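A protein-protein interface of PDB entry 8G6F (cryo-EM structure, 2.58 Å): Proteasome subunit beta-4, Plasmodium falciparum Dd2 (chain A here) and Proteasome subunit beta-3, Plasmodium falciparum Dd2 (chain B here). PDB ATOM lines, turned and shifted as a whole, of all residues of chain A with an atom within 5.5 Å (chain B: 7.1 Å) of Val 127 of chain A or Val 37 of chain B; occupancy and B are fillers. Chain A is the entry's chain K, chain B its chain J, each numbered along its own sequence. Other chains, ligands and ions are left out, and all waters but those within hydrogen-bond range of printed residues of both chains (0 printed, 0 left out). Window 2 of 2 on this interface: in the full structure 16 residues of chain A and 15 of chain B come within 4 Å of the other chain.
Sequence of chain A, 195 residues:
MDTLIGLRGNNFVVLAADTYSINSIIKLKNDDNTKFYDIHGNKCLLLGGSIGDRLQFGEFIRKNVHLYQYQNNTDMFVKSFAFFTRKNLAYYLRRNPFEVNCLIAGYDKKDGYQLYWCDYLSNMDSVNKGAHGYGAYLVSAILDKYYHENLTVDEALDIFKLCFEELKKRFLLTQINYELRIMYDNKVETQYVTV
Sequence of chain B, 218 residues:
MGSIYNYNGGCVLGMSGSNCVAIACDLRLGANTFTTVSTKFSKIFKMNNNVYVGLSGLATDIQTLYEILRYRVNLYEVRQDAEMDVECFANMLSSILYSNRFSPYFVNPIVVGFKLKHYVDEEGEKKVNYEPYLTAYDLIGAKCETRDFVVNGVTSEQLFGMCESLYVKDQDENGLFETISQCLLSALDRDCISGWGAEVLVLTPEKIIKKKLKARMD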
ATOM      1  N   ARG A   8      11.689  -1.542 -32.082  1.00  0.00           N
ATOM      2  CA  ARG A   8      10.249  -1.392 -32.224  1.00  0.00           C
ATOM      3  C   ARG A   8       9.921  -1.021 -33.658  1.00  0.00           C
ATOM      4  O   ARG A   8      10.466  -0.052 -34.194  1.00  0.00           O
ATOM      5  CB  ARG A   8       9.710  -0.329 -31.270  1.00  0.00           C
ATOM      6  CG  ARG A   8       8.201  -0.273 -31.191  1.00  0.00           C
ATOM      7  CD  ARG A   8       7.732   1.138 -30.935  1.00  0.00           C
ATOM      8  NE  ARG A   8       7.804   1.956 -32.136  1.00  0.00           N
ATOM      9  CZ  ARG A   8       6.895   1.960 -33.100  1.00  0.00           C
ATOM     10  NH1 ARG A   8       5.800   1.226 -33.022  1.00  0.00           N
ATOM     11  NH2 ARG A   8       7.093   2.720 -34.172  1.00  0.00           N
ATOM     12  N   LEU A 115       7.915   0.261 -27.030  1.00  0.00           N
ATOM     13  CA  LEU A 115       9.202  -0.035 -26.422  1.00  0.00           C
ATOM     14  C   LEU A 115       9.644   1.170 -25.609  1.00  0.00           C
ATOM     15  O   LEU A 115       9.624   2.297 -26.108  1.00  0.00           O
ATOM     16  CB  LEU A 115      10.249  -0.370 -27.489  1.00  0.00           C
ATOM     17  CG  LEU A 115      11.692  -0.555 -27.023  1.00  0.00           C
ATOM     18  CD1 LEU A 115      11.853  -1.860 -26.268  1.00  0.00           C
ATOM     19  CD2 LEU A 115      12.625  -0.500 -28.208  1.00  0.00           C
ATOM     20  N   TYR A 116      10.045   0.931 -24.366  1.00  0.00           N
ATOM     21  CA  TYR A 116      10.511   1.968 -23.460  1.00  0.00           C
ATOM     22  C   TYR A 116      11.900   1.620 -22.955  1.00  0.00           C
ATOM     23  O   TYR A 116      12.184   0.465 -22.630  1.00  0.00           O
ATOM     24  CB  TYR A 116       9.567   2.138 -22.269  1.00  0.00           C
ATOM     25  CG  TYR A 116       8.208   2.678 -22.627  1.00  0.00           C
ATOM     26  CD1 TYR A 116       7.225   1.848 -23.134  1.00  0.00           C
ATOM     27  CD2 TYR A 116       7.905   4.018 -22.447  1.00  0.00           C
ATOM     28  CE1 TYR A 116       5.984   2.335 -23.458  1.00  0.00           C
ATOM     29  CE2 TYR A 116       6.666   4.513 -22.765  1.00  0.00           C
ATOM     30  CZ  TYR A 116       5.710   3.668 -23.271  1.00  0.00           C
ATOM     31  OH  TYR A 116       4.471   4.157 -23.596  1.00  0.00           O
ATOM     32  N   TRP A 117      12.750   2.639 -22.881  1.00  0.00           N
ATOM     33  CA  TRP A 117      14.128   2.529 -22.428  1.00  0.00           C
ATOM     34  C   TRP A 117      14.225   3.189 -21.062  1.00  0.00           C
ATOM     35  O   TRP A 117      13.781   4.326 -20.898  1.00  0.00           O
ATOM     36  CB  TRP A 117      15.052   3.211 -23.441  1.00  0.00           C
ATOM     37  CG  TRP A 117      16.521   3.217 -23.132  1.00  0.00           C
ATOM     38  CD1 TRP A 117      17.464   2.391 -23.656  1.00  0.00           C
ATOM     39  CD2 TRP A 117      17.216   4.118 -22.265  1.00  0.00           C
ATOM     40  NE1 TRP A 117      18.698   2.709 -23.163  1.00  0.00           N
ATOM     41  CE2 TRP A 117      18.573   3.766 -22.304  1.00  0.00           C
ATOM     42  CE3 TRP A 117      16.820   5.181 -21.452  1.00  0.00           C
ATOM     43  CZ2 TRP A 117      19.537   4.435 -21.561  1.00  0.00           C
ATOM     44  CZ3 TRP A 117      17.774   5.840 -20.717  1.00  0.00           C
ATOM     45  CH2 TRP A 117      19.118   5.470 -20.779  1.00  0.00           C
ATOM     46  N   ASP A 125      12.023   6.826 -21.410  1.00  0.00           N
ATOM     47  CA  ASP A 125      11.398   7.437 -22.573  1.00  0.00           C
ATOM     48  C   ASP A 125      11.106   6.349 -23.592  1.00  0.00           C
ATOM     49  O   ASP A 125      11.865   5.388 -23.718  1.00  0.00           O
ATOM     50  CB  ASP A 125      12.286   8.521 -23.192  1.00  0.00           C
ATOM     51  CG  ASP A 125      11.532   9.400 -24.169  1.00  0.00           C
ATOM     52  OD1 ASP A 125      10.379   9.771 -23.869  1.00  0.00           O
ATOM     53  OD2 ASP A 125      12.087   9.719 -25.237  1.00  0.00           O
ATOM     54  N   SER A 126       9.996   6.503 -24.305  1.00  0.00           N
ATOM     55  CA  SER A 126       9.649   5.573 -25.367  1.00  0.00           C
ATOM     56  C   SER A 126      10.552   5.801 -26.567  1.00  0.00           C
ATOM     57  O   SER A 126      10.821   6.939 -26.954  1.00  0.00           O
ATOM     58  CB  SER A 126       8.186   5.735 -25.773  1.00  0.00           C
ATOM     59  OG  SER A 126       7.950   7.007 -26.333  1.00  0.00           O
ATOM     60  N   VAL A 127      11.025   4.705 -27.156  1.00  0.00           N
ATOM     61  CA  VAL A 127      11.992   4.758 -28.241  1.00  0.00           C
ATOM     62  C   VAL A 127      11.597   3.754 -29.311  1.00  0.00           C
ATOM     63  O   VAL A 127      10.804   2.842 -29.079  1.00  0.00           O
ATOM     64  CB  VAL A 127      13.424   4.476 -27.743  1.00  0.00           C
ATOM     65  CG1 VAL A 127      13.926   5.640 -26.917  1.00  0.00           C
ATOM     66  CG2 VAL A 127      13.467   3.192 -26.937  1.00  0.00           C
ATOM     67  N   ASN A 128      12.147   3.952 -30.506  1.00  0.00           N
ATOM     68  CA  ASN A 128      12.044   2.962 -31.568  1.00  0.00           C
ATOM     69  C   ASN A 128      13.156   1.931 -31.506  1.00  0.00           C
ATOM     70  O   ASN A 128      12.977   0.813 -31.998  1.00  0.00           O
ATOM     71  CB  ASN A 128      12.073   3.644 -32.937  1.00  0.00           C
ATOM     72  CG  ASN A 128      10.778   4.344 -33.263  1.00  0.00           C
ATOM     73  OD1 ASN A 128       9.700   3.849 -32.952  1.00  0.00           O
ATOM     74  ND2 ASN A 128      10.876   5.505 -33.890  1.00  0.00           N
ATOM     75  N   LYS A 129      14.295   2.282 -30.926  1.00  0.00           N
ATOM     76  CA  LYS A 129      15.390   1.348 -30.747  1.00  0.00           C
ATOM     77  C   LYS A 129      16.207   1.800 -29.550  1.00  0.00           C
ATOM     78  O   LYS A 129      16.385   2.998 -29.331  1.00  0.00           O
ATOM     79  CB  LYS A 129      16.262   1.260 -32.002  1.00  0.00           C
ATOM     80  CG  LYS A 129      17.012   2.524 -32.330  1.00  0.00           C
ATOM     81  CD  LYS A 129      17.284   2.625 -33.812  1.00  0.00           C
ATOM     82  CE  LYS A 129      16.185   3.365 -34.531  1.00  0.00           C
ATOM     83  NZ  LYS A 129      16.230   4.817 -34.256  1.00  0.00           N
ATOM     84  N   GLY A 130      16.696   0.833 -28.778  1.00  0.00           N
ATOM     85  CA  GLY A 130      17.448   1.140 -27.579  1.00  0.00           C
ATOM     86  C   GLY A 130      18.391   0.016 -27.219  1.00  0.00           C
ATOM     87  O   GLY A 130      18.279  -1.104 -27.715  1.00  0.00           O
ATOM     88  N   ASN B   8      22.259  14.244 -18.051  1.00  0.00           N
ATOM     89  CA  ASN B   8      21.273  14.264 -19.126  1.00  0.00           C
ATOM     90  C   ASN B   8      21.385  15.482 -20.026  1.00  0.00           C
ATOM     91  O   ASN B   8      21.181  15.364 -21.234  1.00  0.00           O
ATOM     92  CB  ASN B   8      19.853  14.216 -18.550  1.00  0.00           C
ATOM     93  CG  ASN B   8      19.477  12.850 -18.023  1.00  0.00           C
ATOM     94  OD1 ASN B   8      19.009  12.724 -16.897  1.00  0.00           O
ATOM     95  ND2 ASN B   8      19.665  11.824 -18.835  1.00  0.00           N
ATOM     96  N   ARG B  28      16.506  16.445 -26.625  1.00  0.00           N
ATOM     97  CA  ARG B  28      17.419  15.337 -26.399  1.00  0.00           C
ATOM     98  C   ARG B  28      17.188  14.690 -25.038  1.00  0.00           C
ATOM     99  O   ARG B  28      16.773  15.340 -24.077  1.00  0.00           O
ATOM    100  CB  ARG B  28      18.863  15.823 -26.489  1.00  0.00           C
ATOM    101  CG  ARG B  28      19.902  14.723 -26.504  1.00  0.00           C
ATOM    102  CD  ARG B  28      20.968  14.934 -25.446  1.00  0.00           C
ATOM    103  NE  ARG B  28      22.232  14.309 -25.814  1.00  0.00           N
ATOM    104  CZ  ARG B  28      23.230  14.078 -24.974  1.00  0.00           C
ATOM    105  NH1 ARG B  28      23.145  14.394 -23.693  1.00  0.00           N
ATOM    106  NH2 ARG B  28      24.345  13.519 -25.429  1.00  0.00           N
ATOM    107  N   LEU B  29      17.454  13.388 -24.968  1.00  0.00           N
ATOM    108  CA  LEU B  29      17.634  12.680 -23.706  1.00  0.00           C
ATOM    109  C   LEU B  29      19.007  12.028 -23.732  1.00  0.00           C
ATOM    110  O   LEU B  29      19.315  11.263 -24.650  1.00  0.00           O
ATOM    111  CB  LEU B  29      16.545  11.632 -23.480  1.00  0.00           C
ATOM    112  CG  LEU B  29      16.683  10.849 -22.171  1.00  0.00           C
ATOM    113  CD1 LEU B  29      16.638  11.780 -20.972  1.00  0.00           C
ATOM    114  CD2 LEU B  29      15.620   9.780 -22.057  1.00  0.00           C
ATOM    115  N   GLY B  30      19.826  12.328 -22.726  1.00  0.00           N
ATOM    116  CA  GLY B  30      21.193  11.870 -22.676  1.00  0.00           C
ATOM    117  C   GLY B  30      21.410  10.790 -21.630  1.00  0.00           C
ATOM    118  O   GLY B  30      20.533  10.448 -20.841  1.00  0.00           O
ATOM    119  N   ALA B  31      22.623  10.248 -21.646  1.00  0.00           N
ATOM    120  CA  ALA B  31      23.049   9.254 -20.675  1.00  0.00           C
ATOM    121  C   ALA B  31      24.562   9.322 -20.570  1.00  0.00           C
ATOM    122  O   ALA B  31      25.255   9.336 -21.586  1.00  0.00           O
ATOM    123  CB  ALA B  31      22.603   7.846 -21.075  1.00  0.00           C
ATOM    124  N   THR B  35      25.972  10.242 -24.308  1.00  0.00           N
ATOM    125  CA  THR B  35      25.256   9.284 -25.135  1.00  0.00           C
ATOM    126  C   THR B  35      23.828   9.771 -25.320  1.00  0.00           C
ATOM    127  O   THR B  35      23.127  10.035 -24.341  1.00  0.00           O
ATOM    128  CB  THR B  35      25.267   7.892 -24.511  1.00  0.00           C
ATOM    129  OG1 THR B  35      26.580   7.595 -24.026  1.00  0.00           O
ATOM    130  CG2 THR B  35      24.864   6.853 -25.532  1.00  0.00           C
ATOM    131  N   THR B  36      23.409   9.899 -26.571  1.00  0.00           N
ATOM    132  CA  THR B  36      22.047  10.296 -26.895  1.00  0.00           C
ATOM    133  C   THR B  36      21.210   9.041 -27.081  1.00  0.00           C
ATOM    134  O   THR B  36      21.495   8.225 -27.960  1.00  0.00           O
ATOM    135  CB  THR B  36      22.024  11.158 -28.154  1.00  0.00           C
ATOM    136  OG1 THR B  36      22.894  12.278 -27.971  1.00  0.00           O
ATOM    137  CG2 THR B  36      20.622  11.656 -28.441  1.00  0.00           C
ATOM    138  N   VAL B  37      20.189   8.883 -26.245  1.00  0.00           N
ATOM    139  CA  VAL B  37      19.315   7.727 -26.318  1.00  0.00           C
ATOM    140  C   VAL B  37      17.964   8.064 -26.936  1.00  0.00           C
ATOM    141  O   VAL B  37      17.356   7.194 -27.569  1.00  0.00           O
ATOM    142  CB  VAL B  37      19.135   7.096 -24.922  1.00  0.00           C
ATOM    143  CG1 VAL B  37      20.486   6.819 -24.296  1.00  0.00           C
ATOM    144  CG2 VAL B  37      18.317   7.993 -24.026  1.00  0.00           C
ATOM    145  N   SER B  38      17.486   9.294 -26.791  1.00  0.00           N
ATOM    146  CA  SER B  38      16.242   9.727 -27.402  1.00  0.00           C
ATOM    147  C   SER B  38      16.432  11.096 -28.029  1.00  0.00           C
ATOM    148  O   SER B  38      17.286  11.878 -27.609  1.00  0.00           O
ATOM    149  CB  SER B  38      15.102   9.785 -26.383  1.00  0.00           C
ATOM    150  OG  SER B  38      13.852   9.907 -27.033  1.00  0.00           O
ATOM    151  N   THR B  39      15.625  11.372 -29.053  1.00  0.00           N
ATOM    152  CA  THR B  39      15.578  12.681 -29.691  1.00  0.00           C
ATOM    153  C   THR B  39      14.162  13.243 -29.703  1.00  0.00           C
ATOM    154  O   THR B  39      13.844  14.085 -30.545  1.00  0.00           O
ATOM    155  CB  THR B  39      16.120  12.612 -31.119  1.00  0.00           C
ATOM    156  OG1 THR B  39      15.288  11.751 -31.902  1.00  0.00           O
ATOM    157  CG2 THR B  39      17.536  12.082 -31.130  1.00  0.00           C
ATOM    158  N   LYS B  40      13.296  12.774 -28.803  1.00  0.00           N
ATOM    159  CA  LYS B  40      11.934  13.279 -28.701  1.00  0.00           C
ATOM    160  C   LYS B  40      11.502  13.408 -27.248  1.00  0.00           C
ATOM    161  O   LYS B  40      10.319  13.252 -26.934  1.00  0.00           O
ATOM    162  CB  LYS B  40      10.955  12.382 -29.458  1.00  0.00           C
ATOM    163  CG  LYS B  40      10.912  10.950 -28.963  1.00  0.00           C
ATOM    164  CD  LYS B  40       9.634  10.247 -29.378  1.00  0.00           C
ATOM    165  CE  LYS B  40       9.043   9.446 -28.239  1.00  0.00           C
ATOM    166  NZ  LYS B  40       8.587  10.312 -27.124  1.00  0.00           N
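Of the printed residues of chain B, Ser 126 of chain A touches Lys 40 (3.3 Å). Of chain B, only Val 37 comes within 4 Å of Val 127 of chain A. Of the printed residues of chain A, Val 37 of chain B touches Trp 117 (3.8 Å) and Val 127 (3.8 Å). Of the printed residues of chain A, Ser 38 of chain B touches Asp 125 (2.5 Å). Of the printed residues of chain A, Lys 40 of chain B touches Asp 125 (3.8 Å) and Ser 126 (3.3 Å). The nearest printed residue of chain A that does not touch Leu 29 of chain B is Trp 117 of chain A (4.7 Å).
Of the 10 printed residues of chain A, 4 touch a printed residue of chain B. Printed residues of chain A that touch a printed residue of chain B: Trp 117, Asp 125, Ser 126 and Val 127. Along chain A the printed residues that touch a printed residue of chain B span positions 117 to 127. Among the printed residues, 6 pairs touch across the chains.
N of Val 37 of chain B lies within hydrogen-bond range of O of Leu 29 of chain B (3.0 Å). The backbone NH of Leu 29 of chain B is in hydrogen-bond range of the backbone carbonyl oxygen of Ser 38 of chain B. The side-chain hydroxyl (OG) of Ser 38 of chain B is in hydrogen-bond range of the backbone NH (N) of Lys 40 of chain B (3.4 Å). The backbone carbonyl oxygen (O) of Leu 115 of chain A is in hydrogen-bond range of the backbone NH (N) of Val 127 of chain A, at 3.0 Å. The backbone NH of Trp 117 of chain A lies within hydrogen-bond range of the backbone carbonyl oxygen of Asp 125 of chain A, at 3.0 Å.
Val 37 of chain B touches Trp 117 of chain A. CD2 of Leu 29 of chain B touches CB of Asp 125 of chain A, 3.7 Å away. Val 37 of chain B touches Val 127 of chain A.
The side-chain hydroxyl of Ser 38 of chain B sits at hydrogen-bond distance from the side-chain carboxylate of Asp 125 of chain A, 2.5 Å away. OD1 of Asp 125 of chain A lies within salt-bridge range of NZ of Lys 40 of chain B (3.8 Å). NZ of Lys 40 of chain B lies close to OG of Ser 126 of chain A (3.5 Å).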
